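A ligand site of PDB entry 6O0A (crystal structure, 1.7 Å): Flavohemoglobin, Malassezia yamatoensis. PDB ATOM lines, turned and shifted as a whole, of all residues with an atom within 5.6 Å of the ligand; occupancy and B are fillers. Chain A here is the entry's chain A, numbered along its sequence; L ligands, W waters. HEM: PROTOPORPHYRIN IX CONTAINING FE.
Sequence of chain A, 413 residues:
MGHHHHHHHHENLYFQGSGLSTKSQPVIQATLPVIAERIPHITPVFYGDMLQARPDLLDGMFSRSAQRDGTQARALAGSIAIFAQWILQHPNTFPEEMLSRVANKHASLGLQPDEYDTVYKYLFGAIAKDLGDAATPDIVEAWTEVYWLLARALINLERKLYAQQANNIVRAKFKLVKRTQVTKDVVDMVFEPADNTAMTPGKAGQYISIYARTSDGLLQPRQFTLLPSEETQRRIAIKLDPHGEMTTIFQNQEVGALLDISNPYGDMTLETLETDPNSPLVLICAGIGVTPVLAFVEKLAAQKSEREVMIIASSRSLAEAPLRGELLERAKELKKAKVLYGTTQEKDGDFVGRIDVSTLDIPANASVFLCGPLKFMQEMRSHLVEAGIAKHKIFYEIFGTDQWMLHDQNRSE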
ATOM      1  N   TYR A  47      27.359  30.694 -13.229  1.00  0.00           N
ATOM      2  CA  TYR A  47      25.979  31.154 -13.319  1.00  0.00           C
ATOM      3  C   TYR A  47      25.872  32.477 -14.053  1.00  0.00           C
ATOM      4  O   TYR A  47      24.930  32.683 -14.846  1.00  0.00           O
ATOM      5  CB  TYR A  47      25.366  31.278 -11.924  1.00  0.00           C
ATOM      6  CG  TYR A  47      24.919  29.949 -11.364  1.00  0.00           C
ATOM      7  CD1 TYR A  47      23.854  29.256 -11.937  1.00  0.00           C
ATOM      8  CD2 TYR A  47      25.564  29.384 -10.276  1.00  0.00           C
ATOM      9  CE1 TYR A  47      23.455  28.023 -11.437  1.00  0.00           C
ATOM     10  CE2 TYR A  47      25.172  28.156  -9.770  1.00  0.00           C
ATOM     11  CZ  TYR A  47      24.105  27.480 -10.358  1.00  0.00           C
ATOM     12  OH  TYR A  47      23.706  26.271  -9.843  1.00  0.00           O
ATOM     13  N   MET A  50      26.134  31.559 -17.724  1.00  0.00           N
ATOM     14  CA  MET A  50      24.975  30.801 -18.208  1.00  0.00           C
ATOM     15  C   MET A  50      23.723  31.670 -18.273  1.00  0.00           C
ATOM     16  O   MET A  50      22.970  31.614 -19.244  1.00  0.00           O
ATOM     17  CB  MET A  50      24.716  29.596 -17.306  1.00  0.00           C
ATOM     18  CG  MET A  50      23.499  28.806 -17.779  1.00  0.00           C
ATOM     19  SD  MET A  50      23.375  27.211 -16.957  1.00  0.00           S
ATOM     20  CE  MET A  50      23.200  27.714 -15.241  1.00  0.00           C
ATOM     21  N   LEU A  57      16.293  30.922 -18.330  1.00  0.00           N
ATOM     22  CA  LEU A  57      16.434  30.035 -17.170  1.00  0.00           C
ATOM     23  C   LEU A  57      16.260  30.765 -15.849  1.00  0.00           C
ATOM     24  O   LEU A  57      15.991  30.122 -14.835  1.00  0.00           O
ATOM     25  CB  LEU A  57      17.794  29.326 -17.228  1.00  0.00           C
ATOM     26  CG  LEU A  57      17.955  28.332 -18.389  1.00  0.00           C
ATOM     27  CD1 LEU A  57      19.401  27.802 -18.467  1.00  0.00           C
ATOM     28  CD2 LEU A  57      16.946  27.178 -18.281  1.00  0.00           C
ATOM     29  N   MET A  61      13.123  28.901 -13.686  1.00  0.00           N
ATOM     30  CA  MET A  61      13.920  27.764 -13.246  1.00  0.00           C
ATOM     31  C   MET A  61      14.798  28.152 -12.056  1.00  0.00           C
ATOM     32  O   MET A  61      14.498  27.746 -10.929  1.00  0.00           O
ATOM     33  CB  MET A  61      14.736  27.225 -14.422  1.00  0.00           C
ATOM     34  CG  MET A  61      15.726  26.121 -14.073  1.00  0.00           C
ATOM     35  SD  MET A  61      14.933  24.529 -13.817  1.00  0.00           S
ATOM     36  CE  MET A  61      14.565  24.086 -15.517  1.00  0.00           C
ATOM     37  N   PHE A  62      15.850  28.928 -12.250  1.00  0.00           N
ATOM     38  CA  PHE A  62      16.758  29.271 -11.152  1.00  0.00           C
ATOM     39  C   PHE A  62      16.217  30.394 -10.271  1.00  0.00           C
ATOM     40  O   PHE A  62      15.610  31.356 -10.749  1.00  0.00           O
ATOM     41  CB  PHE A  62      18.128  29.681 -11.705  1.00  0.00           C
ATOM     42  CG  PHE A  62      18.918  28.540 -12.241  1.00  0.00           C
ATOM     43  CD1 PHE A  62      19.598  27.691 -11.379  1.00  0.00           C
ATOM     44  CD2 PHE A  62      18.970  28.298 -13.615  1.00  0.00           C
ATOM     45  CE1 PHE A  62      20.324  26.606 -11.888  1.00  0.00           C
ATOM     46  CE2 PHE A  62      19.681  27.227 -14.119  1.00  0.00           C
ATOM     47  CZ  PHE A  62      20.364  26.383 -13.265  1.00  0.00           C
ATOM     48  N   SER A  63      16.504  30.292  -8.983  1.00  0.00           N
ATOM     49  CA  SER A  63      16.077  31.303  -8.027  1.00  0.00           C
ATOM     50  C   SER A  63      17.051  32.456  -8.012  1.00  0.00           C
ATOM     51  O   SER A  63      18.256  32.260  -7.799  1.00  0.00           O
ATOM     52  CB  SER A  63      15.982  30.712  -6.623  1.00  0.00           C
ATOM     53  OG  SER A  63      15.871  31.765  -5.678  1.00  0.00           O
ATOM     54  N   ALA A  66      18.771  32.699  -4.648  1.00  0.00           N
ATOM     55  CA  ALA A  66      19.876  31.758  -4.454  1.00  0.00           C
ATOM     56  C   ALA A  66      21.128  32.241  -5.156  1.00  0.00           C
ATOM     57  O   ALA A  66      22.244  31.953  -4.700  1.00  0.00           O
ATOM     58  CB  ALA A  66      19.481  30.360  -4.941  1.00  0.00           C
ATOM     59  N   GLN A  67      20.978  33.023  -6.238  1.00  0.00           N
ATOM     60  CA  GLN A  67      22.140  33.633  -6.889  1.00  0.00           C
ATOM     61  C   GLN A  67      22.702  34.772  -6.061  1.00  0.00           C
ATOM     62  O   GLN A  67      23.927  34.903  -5.908  1.00  0.00           O
ATOM     63  CB  GLN A  67      21.745  34.136  -8.279  1.00  0.00           C
ATOM     64  CG  GLN A  67      21.400  33.024  -9.242  1.00  0.00           C
ATOM     65  CD  GLN A  67      22.592  32.137  -9.498  1.00  0.00           C
ATOM     66  OE1 GLN A  67      23.695  32.641  -9.723  1.00  0.00           O
ATOM     67  NE2 GLN A  67      22.409  30.830  -9.414  1.00  0.00           N
ATOM     68  N   ALA A  73      23.720  28.828  -4.150  1.00  0.00           N
ATOM     69  CA  ALA A  73      23.998  28.408  -5.528  1.00  0.00           C
ATOM     70  C   ALA A  73      25.235  27.526  -5.657  1.00  0.00           C
ATOM     71  O   ALA A  73      25.399  26.853  -6.679  1.00  0.00           O
ATOM     72  CB  ALA A  73      24.163  29.644  -6.414  1.00  0.00           C
ATOM     73  N   ALA A  75      25.716  24.805  -4.348  1.00  0.00           N
ATOM     74  CA  ALA A  75      25.373  23.411  -4.125  1.00  0.00           C
ATOM     75  C   ALA A  75      25.583  22.568  -5.383  1.00  0.00           C
ATOM     76  O   ALA A  75      26.019  21.413  -5.296  1.00  0.00           O
ATOM     77  CB  ALA A  75      23.931  23.294  -3.631  1.00  0.00           C
ATOM     78  N   LEU A  76      25.280  23.127  -6.565  1.00  0.00           N
ATOM     79  CA  LEU A  76      25.355  22.357  -7.795  1.00  0.00           C
ATOM     80  C   LEU A  76      26.773  21.870  -8.050  1.00  0.00           C
ATOM     81  O   LEU A  76      27.026  20.672  -8.179  1.00  0.00           O
ATOM     82  CB  LEU A  76      24.849  23.183  -8.995  1.00  0.00           C
ATOM     83  CG  LEU A  76      24.597  22.455 -10.337  1.00  0.00           C
ATOM     84  CD1 LEU A  76      23.607  23.224 -11.234  1.00  0.00           C
ATOM     85  CD2 LEU A  76      25.876  22.154 -11.127  1.00  0.00           C
ATOM     86  N   SER A  79      28.098  19.601  -5.037  1.00  0.00           N
ATOM     87  CA  SER A  79      27.673  18.209  -5.128  1.00  0.00           C
ATOM     88  C   SER A  79      28.538  17.427  -6.112  1.00  0.00           C
ATOM     89  O   SER A  79      28.710  16.219  -5.956  1.00  0.00           O
ATOM     90  CB  SER A  79      26.203  18.135  -5.553  1.00  0.00           C
ATOM     91  OG  SER A  79      26.052  18.577  -6.893  1.00  0.00           O
ATOM     92  N   ILE A  80      29.070  18.091  -7.143  1.00  0.00           N
ATOM     93  CA  ILE A  80      29.957  17.401  -8.074  1.00  0.00           C
ATOM     94  C   ILE A  80      31.248  16.989  -7.362  1.00  0.00           C
ATOM     95  O   ILE A  80      31.781  15.904  -7.602  1.00  0.00           O
ATOM     96  CB  ILE A  80      30.227  18.261  -9.319  1.00  0.00           C
ATOM     97  CG1 ILE A  80      28.920  18.503 -10.093  1.00  0.00           C
ATOM     98  CG2 ILE A  80      31.258  17.605 -10.222  1.00  0.00           C
ATOM     99  CD1 ILE A  80      29.051  19.491 -11.264  1.00  0.00           C
ATOM    100  N   MET A  98      21.849  11.489  -2.006  1.00  0.00           N
ATOM    101  CA  MET A  98      22.011  12.790  -2.646  1.00  0.00           C
ATOM    102  C   MET A  98      21.367  12.810  -4.022  1.00  0.00           C
ATOM    103  O   MET A  98      20.682  13.772  -4.379  1.00  0.00           O
ATOM    104  CB  MET A  98      23.494  13.147  -2.761  1.00  0.00           C
ATOM    105  CG  MET A  98      23.724  14.554  -3.290  1.00  0.00           C
ATOM    106  SD  MET A  98      25.468  14.949  -3.531  1.00  0.00           S
ATOM    107  CE  MET A  98      25.840  13.986  -4.997  1.00  0.00           C
ATOM    108  N   ARG A 101      17.479  13.047  -3.756  1.00  0.00           N
ATOM    109  CA  ARG A 101      17.015  14.369  -3.361  1.00  0.00           C
ATOM    110  C   ARG A 101      17.113  15.351  -4.522  1.00  0.00           C
ATOM    111  O   ARG A 101      16.177  16.107  -4.791  1.00  0.00           O
ATOM    112  CB  ARG A 101      17.820  14.884  -2.163  1.00  0.00           C
ATOM    113  CG  ARG A 101      17.268  16.170  -1.562  1.00  0.00           C
ATOM    114  CD  ARG A 101      18.185  16.728  -0.474  1.00  0.00           C
ATOM    115  NE  ARG A 101      19.483  17.132  -1.005  1.00  0.00           N
ATOM    116  CZ  ARG A 101      20.614  16.462  -0.805  1.00  0.00           C
ATOM    117  NH1 ARG A 101      20.619  15.345  -0.084  1.00  0.00           N
ATOM    118  NH2 ARG A 101      21.750  16.906  -1.336  1.00  0.00           N
ATOM    119  N   VAL A 102      18.250  15.331  -5.230  1.00  0.00           N
ATOM    120  CA  VAL A 102      18.448  16.266  -6.341  1.00  0.00           C
ATOM    121  C   VAL A 102      17.482  15.952  -7.488  1.00  0.00           C
ATOM    122  O   VAL A 102      16.884  16.867  -8.065  1.00  0.00           O
ATOM    123  CB  VAL A 102      19.909  16.223  -6.819  1.00  0.00           C
ATOM    124  CG1 VAL A 102      20.073  17.099  -8.037  1.00  0.00           C
ATOM    125  CG2 VAL A 102      20.838  16.699  -5.705  1.00  0.00           C
ATOM    126  N   LYS A 105      13.996  17.280  -6.752  1.00  0.00           N
ATOM    127  CA  LYS A 105      13.955  18.738  -6.921  1.00  0.00           C
ATOM    128  C   LYS A 105      13.942  19.113  -8.393  1.00  0.00           C
ATOM    129  O   LYS A 105      13.141  19.953  -8.824  1.00  0.00           O
ATOM    130  CB  LYS A 105      15.145  19.385  -6.216  1.00  0.00           C
ATOM    131  CG  LYS A 105      15.134  20.909  -6.224  1.00  0.00           C
ATOM    132  CD  LYS A 105      13.955  21.436  -5.422  1.00  0.00           C
ATOM    133  CE  LYS A 105      14.113  21.140  -3.929  1.00  0.00           C
ATOM    134  NZ  LYS A 105      15.042  22.108  -3.276  1.00  0.00           N
ATOM    135  N   HIS A 106      14.836  18.500  -9.179  1.00  0.00           N
ATOM    136  CA  HIS A 106      14.874  18.758 -10.623  1.00  0.00           C
ATOM    137  C   HIS A 106      13.545  18.465 -11.285  1.00  0.00           C
ATOM    138  O   HIS A 106      13.096  19.217 -12.161  1.00  0.00           O
ATOM    139  CB  HIS A 106      15.948  17.887 -11.258  1.00  0.00           C
ATOM    140  CG  HIS A 106      17.324  18.402 -11.064  1.00  0.00           C
ATOM    141  ND1 HIS A 106      18.448  17.687 -11.441  1.00  0.00           N
ATOM    142  CD2 HIS A 106      17.776  19.571 -10.543  1.00  0.00           C
ATOM    143  CE1 HIS A 106      19.522  18.395 -11.160  1.00  0.00           C
ATOM    144  NE2 HIS A 106      19.142  19.532 -10.597  1.00  0.00           N
ATOM    145  N   LEU A 109      11.001  21.074 -10.672  1.00  0.00           N
ATOM    146  CA  LEU A 109      11.292  22.236 -11.516  1.00  0.00           C
ATOM    147  C   LEU A 109      11.179  21.924 -13.008  1.00  0.00           C
ATOM    148  O   LEU A 109      11.347  22.841 -13.835  1.00  0.00           O
ATOM    149  CB  LEU A 109      12.692  22.754 -11.167  1.00  0.00           C
ATOM    150  CG  LEU A 109      12.812  23.227  -9.708  1.00  0.00           C
ATOM    151  CD1 LEU A 109      14.263  23.329  -9.248  1.00  0.00           C
ATOM    152  CD2 LEU A 109      12.058  24.523  -9.503  1.00  0.00           C
ATOM    153  N   LEU A 111      13.054  19.988 -14.990  1.00  0.00           N
ATOM    154  CA  LEU A 111      14.326  19.977 -15.712  1.00  0.00           C
ATOM    155  C   LEU A 111      14.348  18.924 -16.806  1.00  0.00           C
ATOM    156  O   LEU A 111      14.052  17.745 -16.569  1.00  0.00           O
ATOM    157  CB  LEU A 111      15.476  19.732 -14.733  1.00  0.00           C
ATOM    158  CG  LEU A 111      16.854  19.670 -15.369  1.00  0.00           C
ATOM    159  CD1 LEU A 111      17.160  20.982 -16.093  1.00  0.00           C
ATOM    160  CD2 LEU A 111      17.931  19.351 -14.337  1.00  0.00           C
ATOM    161  N   GLU A 115      19.285  20.159 -20.932  1.00  0.00           N
ATOM    162  CA  GLU A 115      19.923  21.269 -20.232  1.00  0.00           C
ATOM    163  C   GLU A 115      21.192  20.844 -19.498  1.00  0.00           C
ATOM    164  O   GLU A 115      21.947  21.721 -19.064  1.00  0.00           O
ATOM    165  CB  GLU A 115      18.952  21.937 -19.266  1.00  0.00           C
ATOM    166  CG  GLU A 115      17.699  22.496 -19.961  1.00  0.00           C
ATOM    167  CD  GLU A 115      17.978  23.716 -20.846  1.00  0.00           C
ATOM    168  OE1 GLU A 115      19.157  24.119 -21.013  1.00  0.00           O
ATOM    169  OE2 GLU A 115      16.998  24.286 -21.353  1.00  0.00           O
ATOM    170  N   TYR A 116      21.455  19.553 -19.340  1.00  0.00           N
ATOM    171  CA  TYR A 116      22.726  19.161 -18.755  1.00  0.00           C
ATOM    172  C   TYR A 116      23.875  19.551 -19.668  1.00  0.00           C
ATOM    173  O   TYR A 116      24.992  19.806 -19.192  1.00  0.00           O
ATOM    174  CB  TYR A 116      22.748  17.672 -18.454  1.00  0.00           C
ATOM    175  CG  TYR A 116      21.920  17.317 -17.226  1.00  0.00           C
ATOM    176  CD1 TYR A 116      20.554  17.061 -17.342  1.00  0.00           C
ATOM    177  CD2 TYR A 116      22.491  17.261 -15.968  1.00  0.00           C
ATOM    178  CE1 TYR A 116      19.790  16.744 -16.217  1.00  0.00           C
ATOM    179  CE2 TYR A 116      21.751  16.940 -14.850  1.00  0.00           C
ATOM    180  CZ  TYR A 116      20.396  16.688 -14.984  1.00  0.00           C
ATOM    181  OH  TYR A 116      19.652  16.379 -13.873  1.00  0.00           O
ATOM    182  N   THR A 118      23.847  22.369 -21.373  1.00  0.00           N
ATOM    183  CA  THR A 118      23.994  23.793 -21.067  1.00  0.00           C
ATOM    184  C   THR A 118      24.863  24.014 -19.838  1.00  0.00           C
ATOM    185  O   THR A 118      25.808  24.819 -19.864  1.00  0.00           O
ATOM    186  CB  THR A 118      22.607  24.409 -20.845  1.00  0.00           C
ATOM    187  OG1 THR A 118      21.759  24.068 -21.948  1.00  0.00           O
ATOM    188  CG2 THR A 118      22.724  25.928 -20.708  1.00  0.00           C
ATOM    189  N   VAL A 119      24.562  23.303 -18.754  1.00  0.00           N
ATOM    190  CA  VAL A 119      25.347  23.460 -17.541  1.00  0.00           C
ATOM    191  C   VAL A 119      26.786  23.011 -17.766  1.00  0.00           C
ATOM    192  O   VAL A 119      27.724  23.659 -17.308  1.00  0.00           O
ATOM    193  CB  VAL A 119      24.671  22.712 -16.376  1.00  0.00           C
ATOM    194  CG1 VAL A 119      25.659  22.421 -15.257  1.00  0.00           C
ATOM    195  CG2 VAL A 119      23.559  23.595 -15.856  1.00  0.00           C
ATOM    196  N   TYR A 147      31.520  14.666 -14.414  1.00  0.00           N
ATOM    197  CA  TYR A 147      30.271  15.384 -14.680  1.00  0.00           C
ATOM    198  C   TYR A 147      29.265  14.484 -15.376  1.00  0.00           C
ATOM    199  O   TYR A 147      28.085  14.448 -14.995  1.00  0.00           O
ATOM    200  CB  TYR A 147      30.531  16.632 -15.530  1.00  0.00           C
ATOM    201  CG  TYR A 147      29.238  17.379 -15.842  1.00  0.00           C
ATOM    202  CD1 TYR A 147      28.462  17.056 -16.960  1.00  0.00           C
ATOM    203  CD2 TYR A 147      28.768  18.379 -14.991  1.00  0.00           C
ATOM    204  CE1 TYR A 147      27.268  17.732 -17.237  1.00  0.00           C
ATOM    205  CE2 TYR A 147      27.574  19.055 -15.268  1.00  0.00           C
ATOM    206  CZ  TYR A 147      26.829  18.716 -16.374  1.00  0.00           C
ATOM    207  OH  TYR A 147      25.644  19.392 -16.623  1.00  0.00           O
ATOM    208  N   LEU A 150      27.560  11.693 -13.360  1.00  0.00           N
ATOM    209  CA  LEU A 150      26.526  12.237 -12.478  1.00  0.00           C
ATOM    210  C   LEU A 150      25.311  12.693 -13.274  1.00  0.00           C
ATOM    211  O   LEU A 150      24.171  12.382 -12.904  1.00  0.00           O
ATOM    212  CB  LEU A 150      27.132  13.386 -11.679  1.00  0.00           C
ATOM    213  CG  LEU A 150      26.355  14.199 -10.649  1.00  0.00           C
ATOM    214  CD1 LEU A 150      25.694  13.284  -9.643  1.00  0.00           C
ATOM    215  CD2 LEU A 150      27.334  15.115  -9.952  1.00  0.00           C
ATOM    216  N   ALA A 151      25.521  13.417 -14.365  1.00  0.00           N
ATOM    217  CA  ALA A 151      24.408  13.856 -15.201  1.00  0.00           C
ATOM    218  C   ALA A 151      23.590  12.676 -15.695  1.00  0.00           C
ATOM    219  O   ALA A 151      22.351  12.723 -15.682  1.00  0.00           O
ATOM    220  CB  ALA A 151      24.928  14.684 -16.377  1.00  0.00           C
ATOM    221  N   LEU A 154      21.443  11.248 -12.839  1.00  0.00           N
ATOM    222  CA  LEU A 154      20.310  12.118 -12.527  1.00  0.00           C
ATOM    223  C   LEU A 154      19.250  12.070 -13.623  1.00  0.00           C
ATOM    224  O   LEU A 154      18.045  11.997 -13.345  1.00  0.00           O
ATOM    225  CB  LEU A 154      20.796  13.553 -12.329  1.00  0.00           C
ATOM    226  CG  LEU A 154      21.580  13.818 -11.050  1.00  0.00           C
ATOM    227  CD1 LEU A 154      22.163  15.241 -11.060  1.00  0.00           C
ATOM    228  CD2 LEU A 154      20.689  13.588  -9.825  1.00  0.00           C
ATOM    229  N   GLY A 400      14.912  24.589   2.106  1.00  0.00           N
ATOM    230  CA  GLY A 400      15.712  25.525   1.338  1.00  0.00           C
ATOM    231  C   GLY A 400      16.919  24.874   0.699  1.00  0.00           C
ATOM    232  O   GLY A 400      17.068  23.659   0.759  1.00  0.00           O
HETATM  233  CHA HEM L   1      19.280  22.451  -7.474  1.00  0.00           C
HETATM  234  CHB HEM L   1      23.037  19.543  -8.582  1.00  0.00           C
HETATM  235  CHC HEM L   1      22.103  20.163 -13.309  1.00  0.00           C
HETATM  236  CHD HEM L   1      18.824  23.559 -12.191  1.00  0.00           C
HETATM  237  C1A HEM L   1      20.362  21.598  -7.355  1.00  0.00           C
HETATM  238  C2A HEM L   1      20.942  21.112  -6.128  1.00  0.00           C
HETATM  239  C3A HEM L   1      21.974  20.315  -6.438  1.00  0.00           C
HETATM  240  C4A HEM L   1      22.096  20.264  -7.878  1.00  0.00           C
HETATM  241  CMA HEM L   1      22.896  19.566  -5.452  1.00  0.00           C
HETATM  242  CAA HEM L   1      20.433  21.450  -4.714  1.00  0.00           C
HETATM  243  CBA HEM L   1      19.390  20.387  -4.403  1.00  0.00           C
HETATM  244  CGA HEM L   1      18.750  20.658  -3.059  1.00  0.00           C
HETATM  245  O1A HEM L   1      18.295  21.813  -2.837  1.00  0.00           O
HETATM  246  O2A HEM L   1      18.694  19.732  -2.215  1.00  0.00           O
HETATM  247  C1B HEM L   1      23.115  19.443  -9.956  1.00  0.00           C
HETATM  248  C2B HEM L   1      24.066  18.660 -10.707  1.00  0.00           C
HETATM  249  C3B HEM L   1      23.823  18.842 -12.018  1.00  0.00           C
HETATM  250  C4B HEM L   1      22.694  19.732 -12.130  1.00  0.00           C
HETATM  251  CMB HEM L   1      25.171  17.817 -10.039  1.00  0.00           C
HETATM  252  CAB HEM L   1      24.549  18.231 -13.255  1.00  0.00           C
HETATM  253  CBB HEM L   1      25.371  17.171 -13.208  1.00  0.00           C
HETATM  254  C1C HEM L   1      21.159  21.162 -13.406  1.00  0.00           C
HETATM  255  C2C HEM L   1      20.688  21.742 -14.638  1.00  0.00           C
HETATM  256  C3C HEM L   1      19.780  22.684 -14.346  1.00  0.00           C
HETATM  257  C4C HEM L   1      19.659  22.735 -12.906  1.00  0.00           C
HETATM  258  CMC HEM L   1      21.188  21.272 -16.026  1.00  0.00           C
HETATM  259  CAC HEM L   1      18.976  23.635 -15.280  1.00  0.00           C
HETATM  260  CBC HEM L   1      19.443  24.038 -16.468  1.00  0.00           C
HETATM  261  C1D HEM L   1      18.665  23.535 -10.820  1.00  0.00           C
HETATM  262  C2D HEM L   1      17.765  24.404 -10.085  1.00  0.00           C
HETATM  263  C3D HEM L   1      17.895  24.115  -8.791  1.00  0.00           C
HETATM  264  C4D HEM L   1      18.871  23.049  -8.652  1.00  0.00           C
HETATM  265  CMD HEM L   1      16.851  25.460 -10.733  1.00  0.00           C
HETATM  266  CAD HEM L   1      17.113  24.799  -7.647  1.00  0.00           C
HETATM  267  CBD HEM L   1      18.094  25.683  -6.885  1.00  0.00           C
HETATM  268  CGD HEM L   1      18.324  27.001  -7.592  1.00  0.00           C
HETATM  269  O1D HEM L   1      17.333  27.671  -7.992  1.00  0.00           O
HETATM  270  O2D HEM L   1      19.514  27.396  -7.747  1.00  0.00           O
HETATM  271  NA  HEM L   1      21.085  21.059  -8.413  1.00  0.00           N
HETATM  272  NB  HEM L   1      22.285  20.084 -10.859  1.00  0.00           N
HETATM  273  NC  HEM L   1      20.514  21.782 -12.358  1.00  0.00           N
HETATM  274  ND  HEM L   1      19.319  22.721  -9.920  1.00  0.00           N
HETATM  275 FE   HEM L   1      20.629  21.193 -10.390  1.00  0.00          FE
HETATM  276  O   HOH W   1      14.705  27.370  -8.145  1.00  0.00           O
HETATM  277  O   HOH W   2      19.853  29.999  -8.610  1.00  0.00           O
HETATM  278  O   HOH W   3      21.519  25.543  -8.703  1.00  0.00           O
HETATM  279  O   HOH W   4      16.225  21.401  -0.993  1.00  0.00           O
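O of Met 61 touches CMD of the ligand, 3.3 Å away.
Phe 62 touches the ligand.
O of Ala 75 touches CMA of the ligand (3.6 Å).
CG of Leu 76 touches NB of the ligand, at 3.4 Å.
Ser 79 touches the ligand.
Ile 80 touches the ligand (CG1 to CMB, 3.8 Å).
Val 102 touches the ligand (CG2 to CMA, 3.5 Å).
Leu 109 touches the ligand (CD1 to CAD, 3.6 Å).
Leu 111 touches the ligand (CD1 to CAC, 3.3 Å).
O of Glu 115 touches CMC of the ligand (3.2 Å).
Tyr 116 touches the ligand (CE2 to CAB, 3.5 Å).
Val 119 touches the ligand.
Tyr 147 touches the ligand (CE2 to CBB, 3.6 Å).
CD2 of Leu 150 touches CMB of the ligand, 3.5 Å away.
N of Ala 151 touches CBB of the ligand, 3.9 Å away.
Leu 154 touches the ligand (CD1 to C2B, 3.9 Å).
Hydrophobic or aromatic side chains that line the ligand: Met 61, Phe 62, Leu 76, Ile 80, Val 102, His 106, Leu 109, Leu 111, Tyr 116, Val 119, Tyr 147, Leu 150 and Leu 154.
Within 4 Å of the ligand: Met 61, Phe 62, Ser 63, Ala 75, Leu 76, Ser 79, Ile 80, Arg 101, Val 102, Lys 105, His 106, Leu 109, Leu 111, Glu 115, Tyr 116, Val 119, Tyr 147, Leu 150, Ala 151 and Leu 154.
A ring nitrogen (NE2) of His 106 binds an iron atom (FE) of the ligand (2.2 Å).
The backbone NH (N) of Ser 63 is in hydrogen-bond range of an oxygen (O1D) of the ligand, at 2.9 Å.
O2A of the ligand lies within salt-bridge range of NE of Arg 101, 3.0 Å away.
The side-chain amino group of Lys 105 lies within salt-bridge range of an oxygen (O1A) of the ligand (3.3 Å).
The backbone NH (N) of Leu 111 sits at hydrogen-bond distance from the backbone carbonyl oxygen (O) of His 106, 2.9 Å away.
A ring nitrogen (ND1) of His 106 is in hydrogen-bond range of the side-chain hydroxyl (OH) of Tyr 116 (3.0 Å).
The side-chain hydroxyl (OG) of Ser 63 lies within hydrogen-bond range of the backbone NH (N) of Ala 66, 3.2 Å away.
OE1 of Glu 115 sits at hydrogen-bond distance from OG1 of Thr 118 (2.8 Å).
The backbone carbonyl oxygen of Leu 76 sits at hydrogen-bond distance from the side-chain hydroxyl of Ser 79.
The backbone carbonyl oxygen (O) of Ala 75 is in hydrogen-bond range of the side-chain hydroxyl (OG) of Ser 79 (3.3 Å).
The backbone NH (N) of Phe 62 lies within hydrogen-bond range of the backbone carbonyl oxygen (O) of Leu 57 (2.9 Å).
O of Tyr 116 sits at hydrogen-bond distance from OH of Tyr 147.
Water W1 bridges O1D of the ligand (2.6 Å) and O of Met 61 (2.8 Å).
Water W2 lies within hydrogen-bond range of an oxygen (O2D) of the ligand, the side-chain amide nitrogen of Gln 67 and the backbone carbonyl oxygen of Ser 63.
Water W4 lies within hydrogen-bond range of the side-chain amino group (NZ) of Lys 105 (2.7 Å), an oxygen (O1A) of the ligand (2.8 Å) and the backbone carbonyl oxygen (O) of Gly 400 (3.0 Å).
Water W3 lies within hydrogen-bond range of OH of Tyr 47 and O2D of the ligand.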
